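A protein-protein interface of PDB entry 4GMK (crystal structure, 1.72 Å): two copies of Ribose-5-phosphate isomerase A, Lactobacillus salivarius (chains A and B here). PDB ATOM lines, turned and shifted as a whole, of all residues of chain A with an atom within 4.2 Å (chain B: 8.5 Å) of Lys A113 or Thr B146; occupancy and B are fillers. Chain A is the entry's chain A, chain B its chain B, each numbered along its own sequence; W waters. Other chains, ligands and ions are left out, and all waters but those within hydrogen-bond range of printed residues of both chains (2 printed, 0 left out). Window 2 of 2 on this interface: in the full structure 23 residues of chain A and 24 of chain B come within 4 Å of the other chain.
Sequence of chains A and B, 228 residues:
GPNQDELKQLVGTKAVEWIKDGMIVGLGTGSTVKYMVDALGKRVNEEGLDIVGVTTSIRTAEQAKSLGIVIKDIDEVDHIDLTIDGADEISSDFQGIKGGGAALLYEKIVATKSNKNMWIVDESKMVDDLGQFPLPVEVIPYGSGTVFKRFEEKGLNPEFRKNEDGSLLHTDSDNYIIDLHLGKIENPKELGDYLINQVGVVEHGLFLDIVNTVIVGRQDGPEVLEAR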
ATOM      1  N   ILE A  74     -32.563 -18.772 -19.050  1.00  0.00           N
ATOM      2  CA  ILE A  74     -32.618 -20.125 -18.399  1.00  0.00           C
ATOM      3  C   ILE A  74     -31.255 -20.516 -17.784  1.00  0.00           C
ATOM      4  O   ILE A  74     -31.212 -21.283 -16.831  1.00  0.00           O
ATOM      5  CB  ILE A  74     -33.073 -21.181 -19.444  1.00  0.00           C
ATOM      6  CG1 ILE A  74     -33.274 -22.595 -18.799  1.00  0.00           C
ATOM      7  CG2 ILE A  74     -32.022 -21.223 -20.572  1.00  0.00           C
ATOM      8  CD1 ILE A  74     -33.918 -23.601 -19.775  1.00  0.00           C
ATOM      9  N   ASP A  75     -30.146 -19.995 -18.312  1.00  0.00           N
ATOM     10  CA  ASP A  75     -28.877 -20.461 -17.828  1.00  0.00           C
ATOM     11  C   ASP A  75     -28.447 -19.649 -16.582  1.00  0.00           C
ATOM     12  O   ASP A  75     -27.453 -19.992 -15.977  1.00  0.00           O
ATOM     13  CB  ASP A  75     -27.765 -20.348 -18.884  1.00  0.00           C
ATOM     14  CG  ASP A  75     -27.866 -21.427 -20.016  1.00  0.00           C
ATOM     15  OD1 ASP A  75     -28.529 -22.468 -19.807  1.00  0.00           O
ATOM     16  OD2 ASP A  75     -27.291 -21.186 -21.084  1.00  0.00           O
ATOM     17  N   VAL A  77     -30.501 -19.410 -13.940  1.00  0.00           N
ATOM     18  CA  VAL A  77     -31.247 -19.957 -12.816  1.00  0.00           C
ATOM     19  C   VAL A  77     -30.772 -21.390 -12.662  1.00  0.00           C
ATOM     20  O   VAL A  77     -30.501 -22.063 -13.647  1.00  0.00           O
ATOM     21  CB  VAL A  77     -32.797 -19.850 -12.990  1.00  0.00           C
ATOM     22  CG1 VAL A  77     -33.215 -18.417 -13.308  1.00  0.00           C
ATOM     23  CG2 VAL A  77     -33.313 -20.763 -14.120  1.00  0.00           C
ATOM     24  N   ASP A  78     -30.612 -21.854 -11.437  1.00  0.00           N
ATOM     25  CA  ASP A  78     -30.109 -23.224 -11.257  1.00  0.00           C
ATOM     26  C   ASP A  78     -31.172 -24.313 -11.230  1.00  0.00           C
ATOM     27  O   ASP A  78     -30.855 -25.500 -11.233  1.00  0.00           O
ATOM     28  CB  ASP A  78     -29.134 -23.325 -10.067  1.00  0.00           C
ATOM     29  CG  ASP A  78     -29.799 -23.070  -8.747  1.00  0.00           C
ATOM     30  OD1 ASP A  78     -31.026 -22.814  -8.700  1.00  0.00           O
ATOM     31  OD2 ASP A  78     -29.078 -23.118  -7.735  1.00  0.00           O
ATOM     32  N   ILE A  80     -35.767 -24.841 -12.263  1.00  0.00           N
ATOM     33  CA  ILE A  80     -37.064 -24.162 -12.513  1.00  0.00           C
ATOM     34  C   ILE A  80     -38.077 -24.977 -11.735  1.00  0.00           C
ATOM     35  O   ILE A  80     -38.057 -26.199 -11.844  1.00  0.00           O
ATOM     36  CB  ILE A  80     -37.447 -24.086 -14.036  1.00  0.00           C
ATOM     37  CG1 ILE A  80     -36.426 -23.253 -14.811  1.00  0.00           C
ATOM     38  CG2 ILE A  80     -38.885 -23.609 -14.234  1.00  0.00           C
ATOM     39  CD1 ILE A  80     -36.532 -23.326 -16.356  1.00  0.00           C
ATOM     40  N   ILE A 109     -36.858 -27.128 -24.208  1.00  0.00           N
ATOM     41  CA  ILE A 109     -35.659 -26.790 -23.408  1.00  0.00           C
ATOM     42  C   ILE A 109     -36.084 -26.424 -21.973  1.00  0.00           C
ATOM     43  O   ILE A 109     -35.536 -26.970 -20.973  1.00  0.00           O
ATOM     44  CB  ILE A 109     -34.892 -25.653 -24.125  1.00  0.00           C
ATOM     45  CG1 ILE A 109     -34.139 -26.257 -25.312  1.00  0.00           C
ATOM     46  CG2 ILE A 109     -33.847 -25.041 -23.176  1.00  0.00           C
ATOM     47  CD1 ILE A 109     -33.589 -25.132 -26.243  1.00  0.00           C
ATOM     48  N   VAL A 110     -37.081 -25.544 -21.873  1.00  0.00           N
ATOM     49  CA  VAL A 110     -37.552 -25.100 -20.532  1.00  0.00           C
ATOM     50  C   VAL A 110     -38.189 -26.269 -19.726  1.00  0.00           C
ATOM     51  O   VAL A 110     -37.911 -26.468 -18.530  1.00  0.00           O
ATOM     52  CB  VAL A 110     -38.474 -23.871 -20.666  1.00  0.00           C
ATOM     53  CG1 VAL A 110     -39.091 -23.487 -19.306  1.00  0.00           C
ATOM     54  CG2 VAL A 110     -37.629 -22.681 -21.197  1.00  0.00           C
ATOM     55  N   ALA A 111     -39.054 -27.021 -20.403  1.00  0.00           N
ATOM     56  CA  ALA A 111     -39.751 -28.187 -19.792  1.00  0.00           C
ATOM     57  C   ALA A 111     -38.758 -29.194 -19.249  1.00  0.00           C
ATOM     58  O   ALA A 111     -38.949 -29.788 -18.144  1.00  0.00           O
ATOM     59  CB  ALA A 111     -40.709 -28.822 -20.811  1.00  0.00           C
ATOM     60  N   THR A 112     -37.651 -29.365 -19.978  1.00  0.00           N
ATOM     61  CA  THR A 112     -36.638 -30.344 -19.558  1.00  0.00           C
ATOM     62  C   THR A 112     -35.895 -29.917 -18.267  1.00  0.00           C
ATOM     63  O   THR A 112     -35.609 -30.770 -17.407  1.00  0.00           O
ATOM     64  CB  THR A 112     -35.655 -30.582 -20.714  1.00  0.00           C
ATOM     65  OG1 THR A 112     -36.404 -31.110 -21.800  1.00  0.00           O
ATOM     66  CG2 THR A 112     -34.544 -31.618 -20.277  1.00  0.00           C
ATOM     67  N   LYS A 113     -35.678 -28.623 -18.089  1.00  0.00           N
ATOM     68  CA  LYS A 113     -35.081 -28.089 -16.812  1.00  0.00           C
ATOM     69  C   LYS A 113     -36.044 -28.059 -15.648  1.00  0.00           C
ATOM     70  O   LYS A 113     -35.619 -28.038 -14.500  1.00  0.00           O
ATOM     71  CB  LYS A 113     -34.414 -26.730 -17.033  1.00  0.00           C
ATOM     72  CG  LYS A 113     -33.484 -26.271 -15.878  1.00  0.00           C
ATOM     73  CD  LYS A 113     -32.596 -25.106 -16.356  1.00  0.00           C
ATOM     74  CE  LYS A 113     -31.497 -24.910 -15.276  1.00  0.00           C
ATOM     75  NZ  LYS A 113     -30.549 -23.853 -15.759  1.00  0.00           N
ATOM     76  N   SER A 114     -37.325 -28.063 -15.945  1.00  0.00           N
ATOM     77  CA  SER A 114     -38.350 -27.859 -14.926  1.00  0.00           C
ATOM     78  C   SER A 114     -38.599 -29.051 -14.032  1.00  0.00           C
ATOM     79  O   SER A 114     -38.678 -30.208 -14.504  1.00  0.00           O
ATOM     80  CB  SER A 114     -39.650 -27.464 -15.619  1.00  0.00           C
ATOM     81  OG  SER A 114     -39.443 -26.294 -16.350  1.00  0.00           O
ATOM     82  N   ASN A 115     -38.766 -28.781 -12.733  1.00  0.00           N
ATOM     83  CA  ASN A 115     -39.101 -29.868 -11.791  1.00  0.00           C
ATOM     84  C   ASN A 115     -40.501 -30.423 -12.082  1.00  0.00           C
ATOM     85  O   ASN A 115     -40.720 -31.663 -12.073  1.00  0.00           O
ATOM     86  CB  ASN A 115     -39.042 -29.346 -10.357  1.00  0.00           C
ATOM     87  CG  ASN A 115     -37.633 -29.069  -9.878  1.00  0.00           C
ATOM     88  OD1 ASN A 115     -36.666 -29.509 -10.494  1.00  0.00           O
ATOM     89  ND2 ASN A 115     -37.508 -28.315  -8.767  1.00  0.00           N
ATOM     90  N   VAL B 139     -24.736 -27.197 -30.465  1.00  0.00           N
ATOM     91  CA  VAL B 139     -25.721 -26.992 -29.419  1.00  0.00           C
ATOM     92  C   VAL B 139     -26.475 -25.666 -29.641  1.00  0.00           C
ATOM     93  O   VAL B 139     -25.839 -24.637 -29.935  1.00  0.00           O
ATOM     94  CB  VAL B 139     -25.010 -26.977 -28.027  1.00  0.00           C
ATOM     95  CG1 VAL B 139     -25.989 -26.677 -26.924  1.00  0.00           C
ATOM     96  CG2 VAL B 139     -24.324 -28.322 -27.755  1.00  0.00           C
ATOM     97  N   ILE B 140     -27.823 -25.685 -29.493  1.00  0.00           N
ATOM     98  CA  ILE B 140     -28.631 -24.422 -29.526  1.00  0.00           C
ATOM     99  C   ILE B 140     -28.139 -23.440 -28.407  1.00  0.00           C
ATOM    100  O   ILE B 140     -27.980 -23.825 -27.267  1.00  0.00           O
ATOM    101  CB  ILE B 140     -30.142 -24.837 -29.307  1.00  0.00           C
ATOM    102  CG1 ILE B 140     -30.619 -25.677 -30.502  1.00  0.00           C
ATOM    103  CG2 ILE B 140     -31.019 -23.572 -28.996  1.00  0.00           C
ATOM    104  CD1 ILE B 140     -30.745 -24.937 -31.846  1.00  0.00           C
ATOM    105  N   PRO B 141     -27.972 -22.134 -28.724  1.00  0.00           N
ATOM    106  CA  PRO B 141     -27.387 -21.232 -27.746  1.00  0.00           C
ATOM    107  C   PRO B 141     -28.265 -21.151 -26.501  1.00  0.00           C
ATOM    108  O   PRO B 141     -27.744 -21.155 -25.393  1.00  0.00           O
ATOM    109  CB  PRO B 141     -27.300 -19.877 -28.546  1.00  0.00           C
ATOM    110  CG  PRO B 141     -26.949 -20.428 -29.923  1.00  0.00           C
ATOM    111  CD  PRO B 141     -27.910 -21.593 -30.094  1.00  0.00           C
ATOM    112  N   TYR B 142     -29.585 -20.998 -26.652  1.00  0.00           N
ATOM    113  CA  TYR B 142     -30.432 -20.837 -25.473  1.00  0.00           C
ATOM    114  C   TYR B 142     -30.503 -22.115 -24.661  1.00  0.00           C
ATOM    115  O   TYR B 142     -30.926 -23.154 -25.217  1.00  0.00           O
ATOM    116  CB  TYR B 142     -31.856 -20.450 -25.900  1.00  0.00           C
ATOM    117  CG  TYR B 142     -32.820 -20.108 -24.749  1.00  0.00           C
ATOM    118  CD1 TYR B 142     -32.570 -19.004 -23.924  1.00  0.00           C
ATOM    119  CD2 TYR B 142     -34.012 -20.825 -24.566  1.00  0.00           C
ATOM    120  CE1 TYR B 142     -33.440 -18.662 -22.907  1.00  0.00           C
ATOM    121  CE2 TYR B 142     -34.921 -20.484 -23.562  1.00  0.00           C
ATOM    122  CZ  TYR B 142     -34.613 -19.396 -22.738  1.00  0.00           C
ATOM    123  OH  TYR B 142     -35.475 -18.963 -21.729  1.00  0.00           O
ATOM    124  N   GLY B 143     -30.099 -22.034 -23.391  1.00  0.00           N
ATOM    125  CA  GLY B 143     -29.973 -23.284 -22.561  1.00  0.00           C
ATOM    126  C   GLY B 143     -28.637 -24.033 -22.750  1.00  0.00           C
ATOM    127  O   GLY B 143     -28.440 -25.109 -22.162  1.00  0.00           O
ATOM    128  N   SER B 144     -27.728 -23.506 -23.558  1.00  0.00           N
ATOM    129  CA  SER B 144     -26.433 -24.236 -23.802  1.00  0.00           C
ATOM    130  C   SER B 144     -25.583 -24.413 -22.532  1.00  0.00           C
ATOM    131  O   SER B 144     -24.853 -25.407 -22.468  1.00  0.00           O
ATOM    132  CB  SER B 144     -25.640 -23.558 -24.916  1.00  0.00           C
ATOM    133  OG  SER B 144     -25.313 -22.198 -24.593  1.00  0.00           O
ATOM    134  N   GLY B 145     -25.693 -23.472 -21.553  1.00  0.00           N
ATOM    135  CA  GLY B 145     -24.991 -23.610 -20.277  1.00  0.00           C
ATOM    136  C   GLY B 145     -25.530 -24.802 -19.485  1.00  0.00           C
ATOM    137  O   GLY B 145     -24.790 -25.471 -18.766  1.00  0.00           O
ATOM    138  N   THR B 146     -26.845 -25.025 -19.541  1.00  0.00           N
ATOM    139  CA  THR B 146     -27.466 -26.133 -18.875  1.00  0.00           C
ATOM    140  C   THR B 146     -27.079 -27.442 -19.568  1.00  0.00           C
ATOM    141  O   THR B 146     -26.869 -28.460 -18.877  1.00  0.00           O
ATOM    142  CB  THR B 146     -29.011 -25.971 -18.881  1.00  0.00           C
ATOM    143  OG1 THR B 146     -29.313 -24.704 -18.253  1.00  0.00           O
ATOM    144  CG2 THR B 146     -29.693 -27.050 -18.070  1.00  0.00           C
ATOM    145  N   VAL B 147     -27.041 -27.457 -20.894  1.00  0.00           N
ATOM    146  CA  VAL B 147     -26.578 -28.662 -21.622  1.00  0.00           C
ATOM    147  C   VAL B 147     -25.120 -28.964 -21.168  1.00  0.00           C
ATOM    148  O   VAL B 147     -24.769 -30.124 -20.906  1.00  0.00           O
ATOM    149  CB  VAL B 147     -26.564 -28.432 -23.160  1.00  0.00           C
ATOM    150  CG1 VAL B 147     -25.897 -29.640 -23.861  1.00  0.00           C
ATOM    151  CG2 VAL B 147     -28.027 -28.296 -23.649  1.00  0.00           C
ATOM    152  N   PHE B 148     -24.289 -27.945 -21.120  1.00  0.00           N
ATOM    153  CA  PHE B 148     -22.863 -28.094 -20.684  1.00  0.00           C
ATOM    154  C   PHE B 148     -22.803 -28.739 -19.269  1.00  0.00           C
ATOM    155  O   PHE B 148     -22.064 -29.696 -19.029  1.00  0.00           O
ATOM    156  CB  PHE B 148     -22.228 -26.694 -20.583  1.00  0.00           C
ATOM    157  CG  PHE B 148     -20.799 -26.699 -20.220  1.00  0.00           C
ATOM    158  CD1 PHE B 148     -20.396 -26.752 -18.881  1.00  0.00           C
ATOM    159  CD2 PHE B 148     -19.830 -26.625 -21.211  1.00  0.00           C
ATOM    160  CE1 PHE B 148     -19.011 -26.790 -18.555  1.00  0.00           C
ATOM    161  CE2 PHE B 148     -18.449 -26.610 -20.886  1.00  0.00           C
ATOM    162  CZ  PHE B 148     -18.046 -26.661 -19.559  1.00  0.00           C
ATOM    163  N   LYS B 149     -23.658 -28.272 -18.352  1.00  0.00           N
ATOM    164  CA  LYS B 149     -23.710 -28.855 -16.999  1.00  0.00           C
ATOM    165  C   LYS B 149     -24.158 -30.349 -17.014  1.00  0.00           C
ATOM    166  O   LYS B 149     -23.638 -31.173 -16.268  1.00  0.00           O
ATOM    167  CB  LYS B 149     -24.648 -27.996 -16.118  1.00  0.00           C
ATOM    168  CG  LYS B 149     -24.681 -28.464 -14.649  1.00  0.00           C
ATOM    169  CD  LYS B 149     -23.230 -28.567 -14.135  1.00  0.00           C
ATOM    170  CE  LYS B 149     -23.078 -28.441 -12.609  1.00  0.00           C
ATOM    171  NZ  LYS B 149     -23.044 -29.757 -11.910  1.00  0.00           N
ATOM    172  N   ARG B 150     -25.089 -30.695 -17.899  1.00  0.00           N
ATOM    173  CA  ARG B 150     -25.507 -32.095 -17.998  1.00  0.00           C
ATOM    174  C   ARG B 150     -24.305 -32.921 -18.440  1.00  0.00           C
ATOM    175  O   ARG B 150     -24.094 -34.060 -17.936  1.00  0.00           O
ATOM    176  CB  ARG B 150     -26.633 -32.291 -19.017  1.00  0.00           C
ATOM    177  CG  ARG B 150     -27.971 -31.703 -18.492  1.00  0.00           C
ATOM    178  CD  ARG B 150     -29.140 -31.945 -19.459  1.00  0.00           C
ATOM    179  NE  ARG B 150     -30.321 -31.271 -18.893  1.00  0.00           N
ATOM    180  CZ  ARG B 150     -30.930 -30.199 -19.428  1.00  0.00           C
ATOM    181  NH1 ARG B 150     -30.492 -29.667 -20.599  1.00  0.00           N
ATOM    182  NH2 ARG B 150     -31.965 -29.651 -18.741  1.00  0.00           N
ATOM    183  N   PHE B 151     -23.583 -32.416 -19.420  1.00  0.00           N
ATOM    184  CA  PHE B 151     -22.412 -33.150 -19.951  1.00  0.00           C
ATOM    185  C   PHE B 151     -21.289 -33.266 -18.896  1.00  0.00           C
ATOM    186  O   PHE B 151     -20.618 -34.282 -18.829  1.00  0.00           O
ATOM    187  CB  PHE B 151     -21.783 -32.468 -21.186  1.00  0.00           C
ATOM    188  CG  PHE B 151     -22.659 -32.480 -22.432  1.00  0.00           C
ATOM    189  CD1 PHE B 151     -23.784 -33.353 -22.519  1.00  0.00           C
ATOM    190  CD2 PHE B 151     -22.310 -31.659 -23.535  1.00  0.00           C
ATOM    191  CE1 PHE B 151     -24.552 -33.396 -23.711  1.00  0.00           C
ATOM    192  CE2 PHE B 151     -23.059 -31.716 -24.733  1.00  0.00           C
ATOM    193  CZ  PHE B 151     -24.174 -32.566 -24.794  1.00  0.00           C
ATOM    194  N   GLU B 152     -21.117 -32.235 -18.101  1.00  0.00           N
ATOM    195  CA  GLU B 152     -20.109 -32.233 -17.002  1.00  0.00           C
ATOM    196  C   GLU B 152     -20.492 -33.321 -15.978  1.00  0.00           C
ATOM    197  O   GLU B 152     -19.656 -34.162 -15.566  1.00  0.00           O
ATOM    198  CB  GLU B 152     -20.127 -30.815 -16.439  1.00  0.00           C
ATOM    199  CG  GLU B 152     -18.969 -30.367 -15.592  1.00  0.00           C
ATOM    200  CD  GLU B 152     -19.042 -28.840 -15.309  1.00  0.00           C
ATOM    201  OE1 GLU B 152     -20.147 -28.210 -15.345  1.00  0.00           O
ATOM    202  OE2 GLU B 152     -17.974 -28.254 -15.111  1.00  0.00           O
ATOM    203  N   GLU B 153     -21.779 -33.401 -15.617  1.00  0.00           N
ATOM    204  CA  GLU B 153     -22.268 -34.388 -14.649  1.00  0.00           C
ATOM    205  C   GLU B 153     -22.152 -35.819 -15.144  1.00  0.00           C
ATOM    206  O   GLU B 153     -21.860 -36.748 -14.350  1.00  0.00           O
ATOM    207  CB  GLU B 153     -23.718 -34.017 -14.202  1.00  0.00           C
ATOM    208  CG  GLU B 153     -23.650 -32.756 -13.358  1.00  0.00           C
ATOM    209  CD  GLU B 153     -24.970 -32.328 -12.728  1.00  0.00           C
ATOM    210  OE1 GLU B 153     -26.044 -32.844 -13.106  1.00  0.00           O
ATOM    211  OE2 GLU B 153     -24.935 -31.432 -11.844  1.00  0.00           O
ATOM    212  N   PHE B 160     -16.515 -25.344 -24.180  1.00  0.00           N
ATOM    213  CA  PHE B 160     -17.036 -24.585 -25.315  1.00  0.00           C
ATOM    214  C   PHE B 160     -15.943 -24.195 -26.315  1.00  0.00           C
ATOM    215  O   PHE B 160     -14.826 -23.831 -25.921  1.00  0.00           O
ATOM    216  CB  PHE B 160     -17.696 -23.254 -24.842  1.00  0.00           C
ATOM    217  CG  PHE B 160     -19.112 -23.420 -24.403  1.00  0.00           C
ATOM    218  CD1 PHE B 160     -20.126 -23.424 -25.344  1.00  0.00           C
ATOM    219  CD2 PHE B 160     -19.422 -23.587 -23.079  1.00  0.00           C
ATOM    220  CE1 PHE B 160     -21.467 -23.540 -24.952  1.00  0.00           C
ATOM    221  CE2 PHE B 160     -20.724 -23.736 -22.673  1.00  0.00           C
ATOM    222  CZ  PHE B 160     -21.770 -23.730 -23.606  1.00  0.00           C
ATOM    223  N   ILE B 178     -19.765 -27.538 -28.323  1.00  0.00           N
ATOM    224  CA  ILE B 178     -19.171 -27.972 -27.072  1.00  0.00           C
ATOM    225  C   ILE B 178     -18.297 -29.153 -27.503  1.00  0.00           C
ATOM    226  O   ILE B 178     -18.834 -30.128 -28.089  1.00  0.00           O
ATOM    227  CB  ILE B 178     -20.207 -28.419 -26.013  1.00  0.00           C
ATOM    228  CG1 ILE B 178     -21.051 -27.179 -25.576  1.00  0.00           C
ATOM    229  CG2 ILE B 178     -19.443 -29.040 -24.814  1.00  0.00           C
ATOM    230  CD1 ILE B 178     -22.238 -27.486 -24.670  1.00  0.00           C
ATOM    231  N   TYR B 194     -27.093 -41.199 -26.870  1.00  0.00           N
ATOM    232  CA  TYR B 194     -27.252 -40.304 -25.719  1.00  0.00           C
ATOM    233  C   TYR B 194     -27.295 -38.833 -26.196  1.00  0.00           C
ATOM    234  O   TYR B 194     -28.198 -38.051 -25.824  1.00  0.00           O
ATOM    235  CB  TYR B 194     -26.062 -40.478 -24.751  1.00  0.00           C
ATOM    236  CG  TYR B 194     -26.044 -39.374 -23.741  1.00  0.00           C
ATOM    237  CD1 TYR B 194     -27.005 -39.335 -22.685  1.00  0.00           C
ATOM    238  CD2 TYR B 194     -25.128 -38.314 -23.873  1.00  0.00           C
ATOM    239  CE1 TYR B 194     -27.051 -38.241 -21.809  1.00  0.00           C
ATOM    240  CE2 TYR B 194     -25.164 -37.255 -22.992  1.00  0.00           C
ATOM    241  CZ  TYR B 194     -26.120 -37.240 -21.967  1.00  0.00           C
ATOM    242  OH  TYR B 194     -26.083 -36.143 -21.132  1.00  0.00           O
ATOM    243  N   GLN B 198     -30.477 -35.684 -26.346  1.00  0.00           N
ATOM    244  CA  GLN B 198     -30.502 -34.517 -25.425  1.00  0.00           C
ATOM    245  C   GLN B 198     -31.119 -33.281 -26.100  1.00  0.00           C
ATOM    246  O   GLN B 198     -30.730 -32.918 -27.238  1.00  0.00           O
ATOM    247  CB  GLN B 198     -29.106 -34.139 -24.998  1.00  0.00           C
ATOM    248  CG  GLN B 198     -28.571 -35.143 -23.947  1.00  0.00           C
ATOM    249  CD  GLN B 198     -29.389 -35.092 -22.681  1.00  0.00           C
ATOM    250  OE1 GLN B 198     -29.885 -36.112 -22.218  1.00  0.00           O
ATOM    251  NE2 GLN B 198     -29.634 -33.886 -22.181  1.00  0.00           N
ATOM    252  N   VAL B 199     -32.101 -32.691 -25.445  1.00  0.00           N
ATOM    253  CA  VAL B 199     -32.752 -31.452 -25.908  1.00  0.00           C
ATOM    254  C   VAL B 199     -31.702 -30.368 -26.136  1.00  0.00           C
ATOM    255  O   VAL B 199     -30.823 -30.136 -25.235  1.00  0.00           O
ATOM    256  CB  VAL B 199     -33.882 -30.998 -24.915  1.00  0.00           C
ATOM    257  CG1 VAL B 199     -33.311 -30.475 -23.597  1.00  0.00           C
ATOM    258  CG2 VAL B 199     -34.828 -29.972 -25.528  1.00  0.00           C
HETATM  259  O   HOH W   1     -32.910 -27.417 -20.188  1.00  0.00           O
HETATM  260  O   HOH W   2     -28.996 -19.518 -22.558  1.00  0.00           O
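No position is printed for both chains.
Of the 12 pairs that touch across the chains among the printed residues, none has its exchanged pair printed and touching as well.
Printed residues of chain B within 4 Å of Lys A113: Thr B146 and Arg B150.
Of the printed residues of chain A, Thr B146 touches Asp A75 and Lys A113.
Of the printed residues of chain B, Ile A109 touches Tyr B142 and Val B199.
Printed residues of chain A within 4 Å of Ser B144: Asp A75 (3.4 Å).
Of the printed residues of chain B, Thr A112 touches Arg B150 (3.6 Å) and Val B199 (3.6 Å).
Of the printed residues of chain A, Val B199 touches Ile A109 (3.7 Å) and Thr A112 (3.6 Å).
Of the printed residues of chain A, Gly B143 touches Ile A74 (3.5 Å) and Asp A75 (3.2 Å).
The nearest printed residue of chain A that does not touch Thr B146 is Ile A74 (4.2 Å).
O of Ile A74 is in hydrogen-bond range of NZ of Lys A113 (2.9 Å).
The side-chain amino group (NZ) of Lys A113 sits at hydrogen-bond distance from the backbone carbonyl oxygen (O) of Val A77 (2.8 Å).
The side-chain hydroxyl (OG) of Ser B144 sits at hydrogen-bond distance from the backbone carbonyl oxygen (O) of Pro B141 (2.8 Å).
CE1 of Tyr B142 touches CG2 of Ile A74, at 3.7 Å.
Ile A74 touches Gly B143 (CG2 to N, 3.5 Å).
Gly B143 touches Asp A75.
Tyr B142 touches Ile A109 (O to CD1, 3.5 Å).
Val B199 touches Ile A109 (CG2 to N, 3.7 Å).
CG2 of Thr A112 touches NH2 of Arg B150 (3.6 Å).
OG1 of Thr A112 touches CG1 of Val B199, 3.6 Å away.
Arg B150 touches Lys A113.
Water W1 bridges the backbone carbonyl oxygen of Ile A109 and the guanidinium group of Arg B150.
Water W2 lies within hydrogen-bond range of OD2 of Asp A75 (2.8 Å) and N of Gly B143 (2.9 Å).
The side-chain carboxylate (OD2) of Asp A75 is in hydrogen-bond range of the backbone NH (N) of Ser B144 (3.4 Å).
N of Gly B145 sits at hydrogen-bond distance from OD2 of Asp A75 (2.8 Å).
The side-chain hydroxyl (OG1) of Thr B146 lies within hydrogen-bond range of the side-chain carboxylate (OD1) of Asp A75, at 2.8 Å.
The side-chain amino group (NZ) of Lys A113 is in hydrogen-bond range of the side-chain hydroxyl (OG1) of Thr B146, at 2.9 Å.
Of the 12 printed residues of chain A, 5 touch a printed residue of chain B.
Hydrophobic or aromatic side chains of chain A that line the printed part of chain B: Ile A74 and Ile A109.
Along chain A the printed residues that touch a printed residue of chain B span positions 74 to 113.
Of the 20 printed residues of chain B, 7 touch a printed residue of chain A.
Hydrophobic or aromatic side chains of chain B within 4 Å of the printed part of chain A: Tyr B142 and Val B199.
Among the printed residues, 12 pairs touch across the chains.
Among the printed residues, no Asp or Glu carboxylate lies within 4 Å of a Lys or Arg side-chain nitrogen of the other chain.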
